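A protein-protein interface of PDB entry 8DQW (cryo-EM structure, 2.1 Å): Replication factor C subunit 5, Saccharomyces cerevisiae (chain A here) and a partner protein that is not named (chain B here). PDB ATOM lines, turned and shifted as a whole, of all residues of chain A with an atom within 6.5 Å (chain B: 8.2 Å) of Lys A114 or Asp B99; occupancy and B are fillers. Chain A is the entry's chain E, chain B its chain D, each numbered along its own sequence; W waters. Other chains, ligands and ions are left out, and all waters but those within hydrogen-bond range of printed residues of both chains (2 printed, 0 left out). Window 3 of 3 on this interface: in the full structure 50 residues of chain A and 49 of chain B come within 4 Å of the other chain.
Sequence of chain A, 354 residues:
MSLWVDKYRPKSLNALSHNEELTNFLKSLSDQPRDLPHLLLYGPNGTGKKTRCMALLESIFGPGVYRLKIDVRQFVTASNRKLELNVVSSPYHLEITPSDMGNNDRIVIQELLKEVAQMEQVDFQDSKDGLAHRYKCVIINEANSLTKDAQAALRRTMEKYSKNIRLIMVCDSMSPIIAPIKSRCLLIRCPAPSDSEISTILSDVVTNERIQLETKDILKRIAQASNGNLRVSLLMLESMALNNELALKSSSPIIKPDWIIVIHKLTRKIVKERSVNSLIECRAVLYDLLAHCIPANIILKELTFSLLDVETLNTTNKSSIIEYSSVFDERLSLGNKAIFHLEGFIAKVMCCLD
The side-chain hydroxyl (OG) of Ser B98 lies within hydrogen-bond range of the side-chain amide oxygen (OD1) of Asn B96 (2.5 Å).
The side-chain carboxylate (OE1) of Glu B141 is in hydrogen-bond range of the backbone NH (N) of Ala B97 (3.0 Å).
The backbone carbonyl oxygen of Ile A109 is in hydrogen-bond range of the backbone NH of Lys A114.
The side-chain hydroxyl of Thr A157 is in hydrogen-bond range of the backbone carbonyl oxygen of Ala A153, at 3.5 Å.
Among the printed residues, pairs that only touch across the chains: Gln A110 with Ser B98 (3.7 Å), Gln A110 with Asp B99 (3.6 Å), Ala A153 with Ala B97 (3.7 Å), Ala A153 with Ser B98 (3.5 Å) and Thr A157 with Ser B98 (3.8 Å).
Water W1 lies within hydrogen-bond range of OE1 of Glu B141, O of Ala A153 and N of Ser B98.
Water W2 bridges O of Ala B97 and NH2 of Arg A106.
The side-chain amide nitrogen (NE2) of Gln A110 is in hydrogen-bond range of the backbone carbonyl oxygen (O) of Ala B97 (3.3 Å).
OG of Ser B98 lies within hydrogen-bond range of NZ of Lys A114 (3.0 Å).
The side-chain amino group (NZ) of Lys A114 lies within salt-bridge range of the side-chain carboxylate (OD1) of Asp B99 (2.7 Å).
Of the 17 printed residues of chain B, 3 touch a printed residue of chain A.
Printed residues of chain B that touch a printed residue of chain A: Ala B97, Ser B98 and Asp B99.
Among the printed residues, Asp or Glu carboxylates within 4 Å of a Lys or Arg side-chain nitrogen of the other chain: Lys A114 with Asp B99 (2.7 Å).
Printed residues of chain B within 4 Å of Gln A110: Ala B97 (3.3 Å), Ser B98 (3.7 Å) and Asp B99 (3.6 Å).
Of the printed residues of chain B, Ala A153 touches Ala B97 (3.7 Å) and Ser B98 (3.5 Å).
Of the printed residues of chain B, Thr A157 touches Ser B98 (3.8 Å).
Of the printed residues of chain A, Ala B97 touches Gln A110 (3.3 Å) and Ala A153 (3.7 Å).
Of the printed residues of chain A, Ser B98 touches Gln A110, Lys A114, Ala A153 and Thr A157.
Of chain A, only Gln A110 (3.6 Å) and Lys A114 (2.7 Å) come within 4 Å of Asp B99.
Gly B102 touches none of the printed residues of chain A.
The nearest residue of chain B that does not touch Lys A114 is Asn B96 (4.7 Å).
The nearest residue of chain A that does not touch Asp B99 is Ala A153 (6.0 Å).
The nearest printed residue of chain B that does not touch Thr A157 is Asn B96 (5.8 Å).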
ATOM      1  N   ARG A 106      20.415 -22.886   0.284  1.00  0.00           N
ATOM      2  CA  ARG A 106      19.541 -22.249   1.264  1.00  0.00           C
ATOM      3  C   ARG A 106      19.885 -22.696   2.679  1.00  0.00           C
ATOM      4  O   ARG A 106      19.887 -21.882   3.612  1.00  0.00           O
ATOM      5  CB  ARG A 106      18.075 -22.549   0.935  1.00  0.00           C
ATOM      6  CG  ARG A 106      17.450 -23.686   1.739  1.00  0.00           C
ATOM      7  CD  ARG A 106      16.111 -24.116   1.159  1.00  0.00           C
ATOM      8  NE  ARG A 106      15.011 -23.295   1.651  1.00  0.00           N
ATOM      9  CZ  ARG A 106      13.755 -23.395   1.235  1.00  0.00           C
ATOM     10  NH1 ARG A 106      13.399 -24.277   0.314  1.00  0.00           N
ATOM     11  NH2 ARG A 106      12.833 -22.590   1.755  1.00  0.00           N
ATOM     12  N   VAL A 108      22.747 -23.384   3.891  1.00  0.00           N
ATOM     13  CA  VAL A 108      23.896 -22.594   4.327  1.00  0.00           C
ATOM     14  C   VAL A 108      23.438 -21.236   4.836  1.00  0.00           C
ATOM     15  O   VAL A 108      23.942 -20.732   5.847  1.00  0.00           O
ATOM     16  CB  VAL A 108      24.912 -22.447   3.179  1.00  0.00           C
ATOM     17  CG1 VAL A 108      26.148 -21.690   3.650  1.00  0.00           C
ATOM     18  CG2 VAL A 108      25.303 -23.801   2.640  1.00  0.00           C
ATOM     19  N   ILE A 109      22.481 -20.620   4.143  1.00  0.00           N
ATOM     20  CA  ILE A 109      21.986 -19.320   4.578  1.00  0.00           C
ATOM     21  C   ILE A 109      21.201 -19.458   5.875  1.00  0.00           C
ATOM     22  O   ILE A 109      21.287 -18.600   6.762  1.00  0.00           O
ATOM     23  CB  ILE A 109      21.136 -18.674   3.468  1.00  0.00           C
ATOM     24  CG1 ILE A 109      21.918 -18.616   2.151  1.00  0.00           C
ATOM     25  CG2 ILE A 109      20.687 -17.281   3.885  1.00  0.00           C
ATOM     26  CD1 ILE A 109      23.283 -17.959   2.260  1.00  0.00           C
ATOM     27  N   GLN A 110      20.429 -20.538   6.012  1.00  0.00           N
ATOM     28  CA  GLN A 110      19.539 -20.667   7.159  1.00  0.00           C
ATOM     29  C   GLN A 110      20.281 -21.062   8.429  1.00  0.00           C
ATOM     30  O   GLN A 110      19.878 -20.655   9.524  1.00  0.00           O
ATOM     31  CB  GLN A 110      18.437 -21.685   6.856  1.00  0.00           C
ATOM     32  CG  GLN A 110      17.384 -21.174   5.884  1.00  0.00           C
ATOM     33  CD  GLN A 110      16.227 -22.137   5.712  1.00  0.00           C
ATOM     34  OE1 GLN A 110      16.409 -23.353   5.736  1.00  0.00           O
ATOM     35  NE2 GLN A 110      15.028 -21.595   5.533  1.00  0.00           N
ATOM     36  N   GLU A 111      21.351 -21.847   8.312  1.00  0.00           N
ATOM     37  CA  GLU A 111      22.087 -22.333   9.474  1.00  0.00           C
ATOM     38  C   GLU A 111      23.354 -21.525   9.737  1.00  0.00           C
ATOM     39  O   GLU A 111      23.505 -20.939  10.813  1.00  0.00           O
ATOM     40  CB  GLU A 111      22.431 -23.818   9.289  1.00  0.00           C
ATOM     41  CG  GLU A 111      21.259 -24.668   8.832  1.00  0.00           C
ATOM     42  CD  GLU A 111      20.038 -24.495   9.714  1.00  0.00           C
ATOM     43  OE1 GLU A 111      20.211 -24.310  10.938  1.00  0.00           O
ATOM     44  OE2 GLU A 111      18.907 -24.538   9.185  1.00  0.00           O
ATOM     45  N   LEU A 112      24.263 -21.464   8.763  1.00  0.00           N
ATOM     46  CA  LEU A 112      25.563 -20.850   9.011  1.00  0.00           C
ATOM     47  C   LEU A 112      25.444 -19.334   9.121  1.00  0.00           C
ATOM     48  O   LEU A 112      25.662 -18.757  10.194  1.00  0.00           O
ATOM     49  CB  LEU A 112      26.541 -21.241   7.898  1.00  0.00           C
ATOM     50  CG  LEU A 112      27.780 -20.359   7.694  1.00  0.00           C
ATOM     51  CD1 LEU A 112      28.608 -20.234   8.968  1.00  0.00           C
ATOM     52  CD2 LEU A 112      28.632 -20.911   6.561  1.00  0.00           C
ATOM     53  N   LEU A 113      25.054 -18.675   8.028  1.00  0.00           N
ATOM     54  CA  LEU A 113      25.063 -17.216   8.007  1.00  0.00           C
ATOM     55  C   LEU A 113      24.246 -16.652   9.162  1.00  0.00           C
ATOM     56  O   LEU A 113      24.722 -15.792   9.913  1.00  0.00           O
ATOM     57  CB  LEU A 113      24.530 -16.706   6.667  1.00  0.00           C
ATOM     58  CG  LEU A 113      24.765 -15.219   6.377  1.00  0.00           C
ATOM     59  CD1 LEU A 113      26.251 -14.887   6.381  1.00  0.00           C
ATOM     60  CD2 LEU A 113      24.134 -14.823   5.053  1.00  0.00           C
ATOM     61  N   LYS A 114      23.021 -17.154   9.339  1.00  0.00           N
ATOM     62  CA  LYS A 114      22.182 -16.672  10.430  1.00  0.00           C
ATOM     63  C   LYS A 114      22.921 -16.763  11.758  1.00  0.00           C
ATOM     64  O   LYS A 114      22.986 -15.786  12.513  1.00  0.00           O
ATOM     65  CB  LYS A 114      20.874 -17.466  10.479  1.00  0.00           C
ATOM     66  CG  LYS A 114      19.882 -16.943  11.508  1.00  0.00           C
ATOM     67  CD  LYS A 114      18.473 -17.454  11.248  1.00  0.00           C
ATOM     68  CE  LYS A 114      17.444 -16.670  12.048  1.00  0.00           C
ATOM     69  NZ  LYS A 114      16.055 -17.154  11.808  1.00  0.00           N
ATOM     70  N   GLU A 115      23.525 -17.921  12.043  1.00  0.00           N
ATOM     71  CA  GLU A 115      24.281 -18.055  13.284  1.00  0.00           C
ATOM     72  C   GLU A 115      25.367 -16.991  13.364  1.00  0.00           C
ATOM     73  O   GLU A 115      25.496 -16.292  14.376  1.00  0.00           O
ATOM     74  CB  GLU A 115      24.886 -19.455  13.393  1.00  0.00           C
ATOM     75  CG  GLU A 115      23.908 -20.521  13.860  1.00  0.00           C
ATOM     76  CD  GLU A 115      24.253 -21.904  13.338  1.00  0.00           C
ATOM     77  OE1 GLU A 115      23.339 -22.601  12.849  1.00  0.00           O
ATOM     78  OE2 GLU A 115      25.437 -22.291  13.416  1.00  0.00           O
ATOM     79  N   VAL A 116      26.129 -16.823  12.280  1.00  0.00           N
ATOM     80  CA  VAL A 116      27.161 -15.791  12.262  1.00  0.00           C
ATOM     81  C   VAL A 116      26.538 -14.430  12.528  1.00  0.00           C
ATOM     82  O   VAL A 116      27.094 -13.608  13.268  1.00  0.00           O
ATOM     83  CB  VAL A 116      27.919 -15.817  10.921  1.00  0.00           C
ATOM     84  CG1 VAL A 116      28.817 -14.593  10.792  1.00  0.00           C
ATOM     85  CG2 VAL A 116      28.729 -17.097  10.792  1.00  0.00           C
ATOM     86  N   ALA A 117      25.371 -14.171  11.936  1.00  0.00           N
ATOM     87  CA  ALA A 117      24.699 -12.899  12.165  1.00  0.00           C
ATOM     88  C   ALA A 117      24.235 -12.763  13.608  1.00  0.00           C
ATOM     89  O   ALA A 117      24.241 -11.656  14.157  1.00  0.00           O
ATOM     90  CB  ALA A 117      23.514 -12.752  11.211  1.00  0.00           C
ATOM     91  N   GLN A 118      23.831 -13.869  14.237  1.00  0.00           N
ATOM     92  CA  GLN A 118      23.275 -13.794  15.583  1.00  0.00           C
ATOM     93  C   GLN A 118      24.351 -13.610  16.645  1.00  0.00           C
ATOM     94  O   GLN A 118      24.116 -12.921  17.643  1.00  0.00           O
ATOM     95  CB  GLN A 118      22.453 -15.050  15.874  1.00  0.00           C
ATOM     96  CG  GLN A 118      21.036 -14.982  15.332  1.00  0.00           C
ATOM     97  CD  GLN A 118      20.297 -16.299  15.450  1.00  0.00           C
ATOM     98  OE1 GLN A 118      20.901 -17.345  15.683  1.00  0.00           O
ATOM     99  NE2 GLN A 118      18.981 -16.254  15.285  1.00  0.00           N
ATOM    100  N   MET A 119      25.526 -14.207  16.452  1.00  0.00           N
ATOM    101  CA  MET A 119      26.608 -14.104  17.426  1.00  0.00           C
ATOM    102  C   MET A 119      27.242 -12.724  17.301  1.00  0.00           C
ATOM    103  O   MET A 119      27.910 -12.426  16.305  1.00  0.00           O
ATOM    104  CB  MET A 119      27.632 -15.213  17.196  1.00  0.00           C
ATOM    105  CG  MET A 119      29.012 -14.956  17.806  1.00  0.00           C
ATOM    106  SD  MET A 119      30.236 -16.208  17.364  1.00  0.00           S
ATOM    107  CE  MET A 119      29.326 -17.721  17.657  1.00  0.00           C
ATOM    108  N   ALA A 153      15.904 -16.120   2.064  1.00  0.00           N
ATOM    109  CA  ALA A 153      16.383 -16.299   3.431  1.00  0.00           C
ATOM    110  C   ALA A 153      17.368 -15.205   3.830  1.00  0.00           C
ATOM    111  O   ALA A 153      17.508 -14.900   5.019  1.00  0.00           O
ATOM    112  CB  ALA A 153      17.031 -17.675   3.584  1.00  0.00           C
ATOM    113  N   THR A 157      17.737 -11.660   7.596  1.00  0.00           N
ATOM    114  CA  THR A 157      19.054 -11.740   8.218  1.00  0.00           C
ATOM    115  C   THR A 157      19.843 -10.460   7.974  1.00  0.00           C
ATOM    116  O   THR A 157      20.467  -9.920   8.895  1.00  0.00           O
ATOM    117  CB  THR A 157      19.819 -12.951   7.686  1.00  0.00           C
ATOM    118  OG1 THR A 157      19.117 -14.152   8.027  1.00  0.00           O
ATOM    119  CG2 THR A 157      21.222 -13.000   8.277  1.00  0.00           C
ATOM    120  N   TYR A 161      19.850  -8.136  11.801  1.00  0.00           N
ATOM    121  CA  TYR A 161      21.180  -8.135  12.411  1.00  0.00           C
ATOM    122  C   TYR A 161      22.163  -7.262  11.635  1.00  0.00           C
ATOM    123  O   TYR A 161      23.282  -7.675  11.341  1.00  0.00           O
ATOM    124  CB  TYR A 161      21.696  -9.564  12.519  1.00  0.00           C
ATOM    125  CG  TYR A 161      20.739 -10.509  13.207  1.00  0.00           C
ATOM    126  CD1 TYR A 161      20.577 -10.482  14.586  1.00  0.00           C
ATOM    127  CD2 TYR A 161      19.998 -11.429  12.479  1.00  0.00           C
ATOM    128  CE1 TYR A 161      19.706 -11.345  15.219  1.00  0.00           C
ATOM    129  CE2 TYR A 161      19.122 -12.295  13.103  1.00  0.00           C
ATOM    130  CZ  TYR A 161      18.979 -12.249  14.473  1.00  0.00           C
ATOM    131  OH  TYR A 161      18.109 -13.110  15.100  1.00  0.00           O
ATOM    132  N   LEU B  93       5.067 -13.804  17.878  1.00  0.00           N
ATOM    133  CA  LEU B  93       5.854 -14.885  17.286  1.00  0.00           C
ATOM    134  C   LEU B  93       6.136 -14.516  15.836  1.00  0.00           C
ATOM    135  O   LEU B  93       5.212 -14.445  15.022  1.00  0.00           O
ATOM    136  CB  LEU B  93       5.129 -16.229  17.379  1.00  0.00           C
ATOM    137  CG  LEU B  93       5.737 -17.362  16.544  1.00  0.00           C
ATOM    138  CD1 LEU B  93       7.171 -17.631  16.974  1.00  0.00           C
ATOM    139  CD2 LEU B  93       4.903 -18.627  16.651  1.00  0.00           C
ATOM    140  N   GLU B  94       7.407 -14.295  15.513  1.00  0.00           N
ATOM    141  CA  GLU B  94       7.824 -13.845  14.191  1.00  0.00           C
ATOM    142  C   GLU B  94       8.534 -14.976  13.457  1.00  0.00           C
ATOM    143  O   GLU B  94       9.459 -15.589  13.999  1.00  0.00           O
ATOM    144  CB  GLU B  94       8.750 -12.631  14.301  1.00  0.00           C
ATOM    145  CG  GLU B  94       8.503 -11.561  13.255  1.00  0.00           C
ATOM    146  CD  GLU B  94       8.791 -12.048  11.849  1.00  0.00           C
ATOM    147  OE1 GLU B  94       9.920 -12.523  11.604  1.00  0.00           O
ATOM    148  OE2 GLU B  94       7.890 -11.958  10.989  1.00  0.00           O
ATOM    149  N   LEU B  95       8.100 -15.248  12.226  1.00  0.00           N
ATOM    150  CA  LEU B  95       8.757 -16.217  11.361  1.00  0.00           C
ATOM    151  C   LEU B  95       8.871 -15.628   9.964  1.00  0.00           C
ATOM    152  O   LEU B  95       7.937 -14.984   9.478  1.00  0.00           O
ATOM    153  CB  LEU B  95       7.989 -17.547  11.312  1.00  0.00           C
ATOM    154  CG  LEU B  95       7.931 -18.359  12.610  1.00  0.00           C
ATOM    155  CD1 LEU B  95       7.085 -19.608  12.414  1.00  0.00           C
ATOM    156  CD2 LEU B  95       9.328 -18.733  13.090  1.00  0.00           C
ATOM    157  N   ASN B  96      10.014 -15.849   9.322  1.00  0.00           N
ATOM    158  CA  ASN B  96      10.281 -15.283   8.005  1.00  0.00           C
ATOM    159  C   ASN B  96      10.991 -16.337   7.159  1.00  0.00           C
ATOM    160  O   ASN B  96      11.119 -17.499   7.555  1.00  0.00           O
ATOM    161  CB  ASN B  96      11.092 -13.986   8.134  1.00  0.00           C
ATOM    162  CG  ASN B  96      12.330 -14.155   8.992  1.00  0.00           C
ATOM    163  OD1 ASN B  96      13.163 -15.022   8.734  1.00  0.00           O
ATOM    164  ND2 ASN B  96      12.456 -13.324  10.020  1.00  0.00           N
ATOM    165  N   ALA B  97      11.461 -15.921   5.981  1.00  0.00           N
ATOM    166  CA  ALA B  97      12.081 -16.856   5.049  1.00  0.00           C
ATOM    167  C   ALA B  97      13.368 -17.458   5.597  1.00  0.00           C
ATOM    168  O   ALA B  97      13.790 -18.520   5.126  1.00  0.00           O
ATOM    169  CB  ALA B  97      12.363 -16.157   3.718  1.00  0.00           C
ATOM    170  N   SER B  98      14.005 -16.812   6.574  1.00  0.00           N
ATOM    171  CA  SER B  98      15.219 -17.361   7.166  1.00  0.00           C
ATOM    172  C   SER B  98      14.937 -18.517   8.117  1.00  0.00           C
ATOM    173  O   SER B  98      15.882 -19.184   8.551  1.00  0.00           O
ATOM    174  CB  SER B  98      15.990 -16.264   7.907  1.00  0.00           C
ATOM    175  OG  SER B  98      15.399 -15.975   9.161  1.00  0.00           O
ATOM    176  N   ASP B  99      13.673 -18.769   8.446  1.00  0.00           N
ATOM    177  CA  ASP B  99      13.286 -19.853   9.335  1.00  0.00           C
ATOM    178  C   ASP B  99      12.685 -21.002   8.538  1.00  0.00           C
ATOM    179  O   ASP B  99      12.069 -20.800   7.488  1.00  0.00           O
ATOM    180  CB  ASP B  99      12.272 -19.368  10.374  1.00  0.00           C
ATOM    181  CG  ASP B  99      12.885 -18.437  11.398  1.00  0.00           C
ATOM    182  OD1 ASP B  99      13.950 -18.780  11.952  1.00  0.00           O
ATOM    183  OD2 ASP B  99      12.302 -17.362  11.646  1.00  0.00           O
ATOM    184  N   GLU B 100      12.875 -22.216   9.044  1.00  0.00           N
ATOM    185  CA  GLU B 100      12.204 -23.372   8.469  1.00  0.00           C
ATOM    186  C   GLU B 100      10.708 -23.284   8.747  1.00  0.00           C
ATOM    187  O   GLU B 100      10.290 -23.062   9.888  1.00  0.00           O
ATOM    188  CB  GLU B 100      12.797 -24.665   9.033  1.00  0.00           C
ATOM    189  CG  GLU B 100      12.311 -25.059  10.425  1.00  0.00           C
ATOM    190  CD  GLU B 100      12.587 -23.998  11.474  1.00  0.00           C
ATOM    191  OE1 GLU B 100      11.641 -23.606  12.188  1.00  0.00           O
ATOM    192  OE2 GLU B 100      13.751 -23.559  11.584  1.00  0.00           O
ATOM    193  N   ARG B 101       9.901 -23.438   7.701  1.00  0.00           N
ATOM    194  CA  ARG B 101       8.453 -23.273   7.797  1.00  0.00           C
ATOM    195  C   ARG B 101       7.741 -24.377   7.021  1.00  0.00           C
ATOM    196  O   ARG B 101       6.795 -24.133   6.271  1.00  0.00           O
ATOM    197  CB  ARG B 101       8.031 -21.894   7.294  1.00  0.00           C
ATOM    198  CG  ARG B 101       8.686 -20.740   8.034  1.00  0.00           C
ATOM    199  CD  ARG B 101       8.044 -19.416   7.672  1.00  0.00           C
ATOM    200  NE  ARG B 101       8.465 -18.941   6.360  1.00  0.00           N
ATOM    201  CZ  ARG B 101       8.161 -17.751   5.861  1.00  0.00           C
ATOM    202  NH1 ARG B 101       7.438 -16.879   6.543  1.00  0.00           N
ATOM    203  NH2 ARG B 101       8.599 -17.427   4.648  1.00  0.00           N
ATOM    204  N   GLY B 102       8.192 -25.612   7.200  1.00  0.00           N
ATOM    205  CA  GLY B 102       7.548 -26.746   6.572  1.00  0.00           C
ATOM    206  C   GLY B 102       6.177 -27.013   7.170  1.00  0.00           C
ATOM    207  O   GLY B 102       5.727 -26.364   8.114  1.00  0.00           O
ATOM    208  N   ILE B 105       6.205 -27.772  10.821  1.00  0.00           N
ATOM    209  CA  ILE B 105       6.369 -26.573  11.637  1.00  0.00           C
ATOM    210  C   ILE B 105       5.027 -25.877  11.819  1.00  0.00           C
ATOM    211  O   ILE B 105       4.650 -25.503  12.935  1.00  0.00           O
ATOM    212  CB  ILE B 105       7.409 -25.632  11.004  1.00  0.00           C
ATOM    213  CG1 ILE B 105       8.780 -26.312  10.955  1.00  0.00           C
ATOM    214  CG2 ILE B 105       7.483 -24.322  11.777  1.00  0.00           C
ATOM    215  CD1 ILE B 105       9.529 -26.285  12.268  1.00  0.00           C
ATOM    216  N   LYS B 109       4.537 -25.909  15.784  1.00  0.00           N
ATOM    217  CA  LYS B 109       5.003 -24.725  16.503  1.00  0.00           C
ATOM    218  C   LYS B 109       4.005 -23.579  16.383  1.00  0.00           C
ATOM    219  O   LYS B 109       3.629 -22.956  17.387  1.00  0.00           O
ATOM    220  CB  LYS B 109       6.378 -24.312  15.974  1.00  0.00           C
ATOM    221  CG  LYS B 109       6.745 -22.853  16.215  1.00  0.00           C
ATOM    222  CD  LYS B 109       8.195 -22.581  15.836  1.00  0.00           C
ATOM    223  CE  LYS B 109       8.663 -21.228  16.344  1.00  0.00           C
ATOM    224  NZ  LYS B 109       9.384 -21.330  17.643  1.00  0.00           N
ATOM    225  N   ILE B 138       3.396 -13.218  13.182  1.00  0.00           N
ATOM    226  CA  ILE B 138       3.806 -12.538  11.962  1.00  0.00           C
ATOM    227  C   ILE B 138       4.509 -13.560  11.080  1.00  0.00           C
ATOM    228  O   ILE B 138       5.470 -14.210  11.512  1.00  0.00           O
ATOM    229  CB  ILE B 138       4.727 -11.345  12.264  1.00  0.00           C
ATOM    230  CG1 ILE B 138       4.015 -10.331  13.162  1.00  0.00           C
ATOM    231  CG2 ILE B 138       5.163 -10.665  10.970  1.00  0.00           C
ATOM    232  CD1 ILE B 138       4.948  -9.313  13.785  1.00  0.00           C
ATOM    233  N   ASP B 140       6.343 -13.185   7.908  1.00  0.00           N
ATOM    234  CA  ASP B 140       6.950 -12.338   6.894  1.00  0.00           C
ATOM    235  C   ASP B 140       7.432 -13.185   5.723  1.00  0.00           C
ATOM    236  O   ASP B 140       7.775 -14.360   5.876  1.00  0.00           O
ATOM    237  CB  ASP B 140       8.115 -11.545   7.490  1.00  0.00           C
ATOM    238  CG  ASP B 140       8.335 -10.213   6.796  1.00  0.00           C
ATOM    239  OD1 ASP B 140       7.684  -9.955   5.761  1.00  0.00           O
ATOM    240  OD2 ASP B 140       9.161  -9.416   7.290  1.00  0.00           O
ATOM    241  N   GLU B 141       7.454 -12.577   4.539  1.00  0.00           N
ATOM    242  CA  GLU B 141       7.814 -13.292   3.317  1.00  0.00           C
ATOM    243  C   GLU B 141       6.953 -14.543   3.163  1.00  0.00           C
ATOM    244  O   GLU B 141       7.436 -15.621   2.812  1.00  0.00           O
ATOM    245  CB  GLU B 141       9.304 -13.645   3.309  1.00  0.00           C
ATOM    246  CG  GLU B 141      10.219 -12.452   3.061  1.00  0.00           C
ATOM    247  CD  GLU B 141      11.216 -12.215   4.184  1.00  0.00           C
ATOM    248  OE1 GLU B 141      11.593 -13.185   4.874  1.00  0.00           O
ATOM    249  OE2 GLU B 141      11.631 -11.053   4.371  1.00  0.00           O
ATOM    250  N   SER B 144       6.908 -17.251   0.261  1.00  0.00           N
ATOM    251  CA  SER B 144       7.874 -18.335   0.131  1.00  0.00           C
ATOM    252  C   SER B 144       7.362 -19.661   0.682  1.00  0.00           C
ATOM    253  O   SER B 144       7.964 -20.701   0.400  1.00  0.00           O
ATOM    254  CB  SER B 144       9.180 -17.966   0.840  1.00  0.00           C
ATOM    255  OG  SER B 144       9.614 -16.669   0.473  1.00  0.00           O
ATOM    256  N   MET B 145       6.279 -19.653   1.455  1.00  0.00           N
ATOM    257  CA  MET B 145       5.750 -20.883   2.024  1.00  0.00           C
ATOM    258  C   MET B 145       5.057 -21.720   0.951  1.00  0.00           C
ATOM    259  O   MET B 145       4.520 -21.197  -0.028  1.00  0.00           O
ATOM    260  CB  MET B 145       4.769 -20.565   3.152  1.00  0.00           C
ATOM    261  CG  MET B 145       5.437 -20.041   4.416  1.00  0.00           C
ATOM    262  SD  MET B 145       4.278 -19.750   5.769  1.00  0.00           S
ATOM    263  CE  MET B 145       3.730 -21.419   6.126  1.00  0.00           C
HETATM  264  O   HOH W   1      14.444 -13.673   5.321  1.00  0.00           O
HETATM  265  O   HOH W   2      14.095 -19.586   2.310  1.00  0.00           O
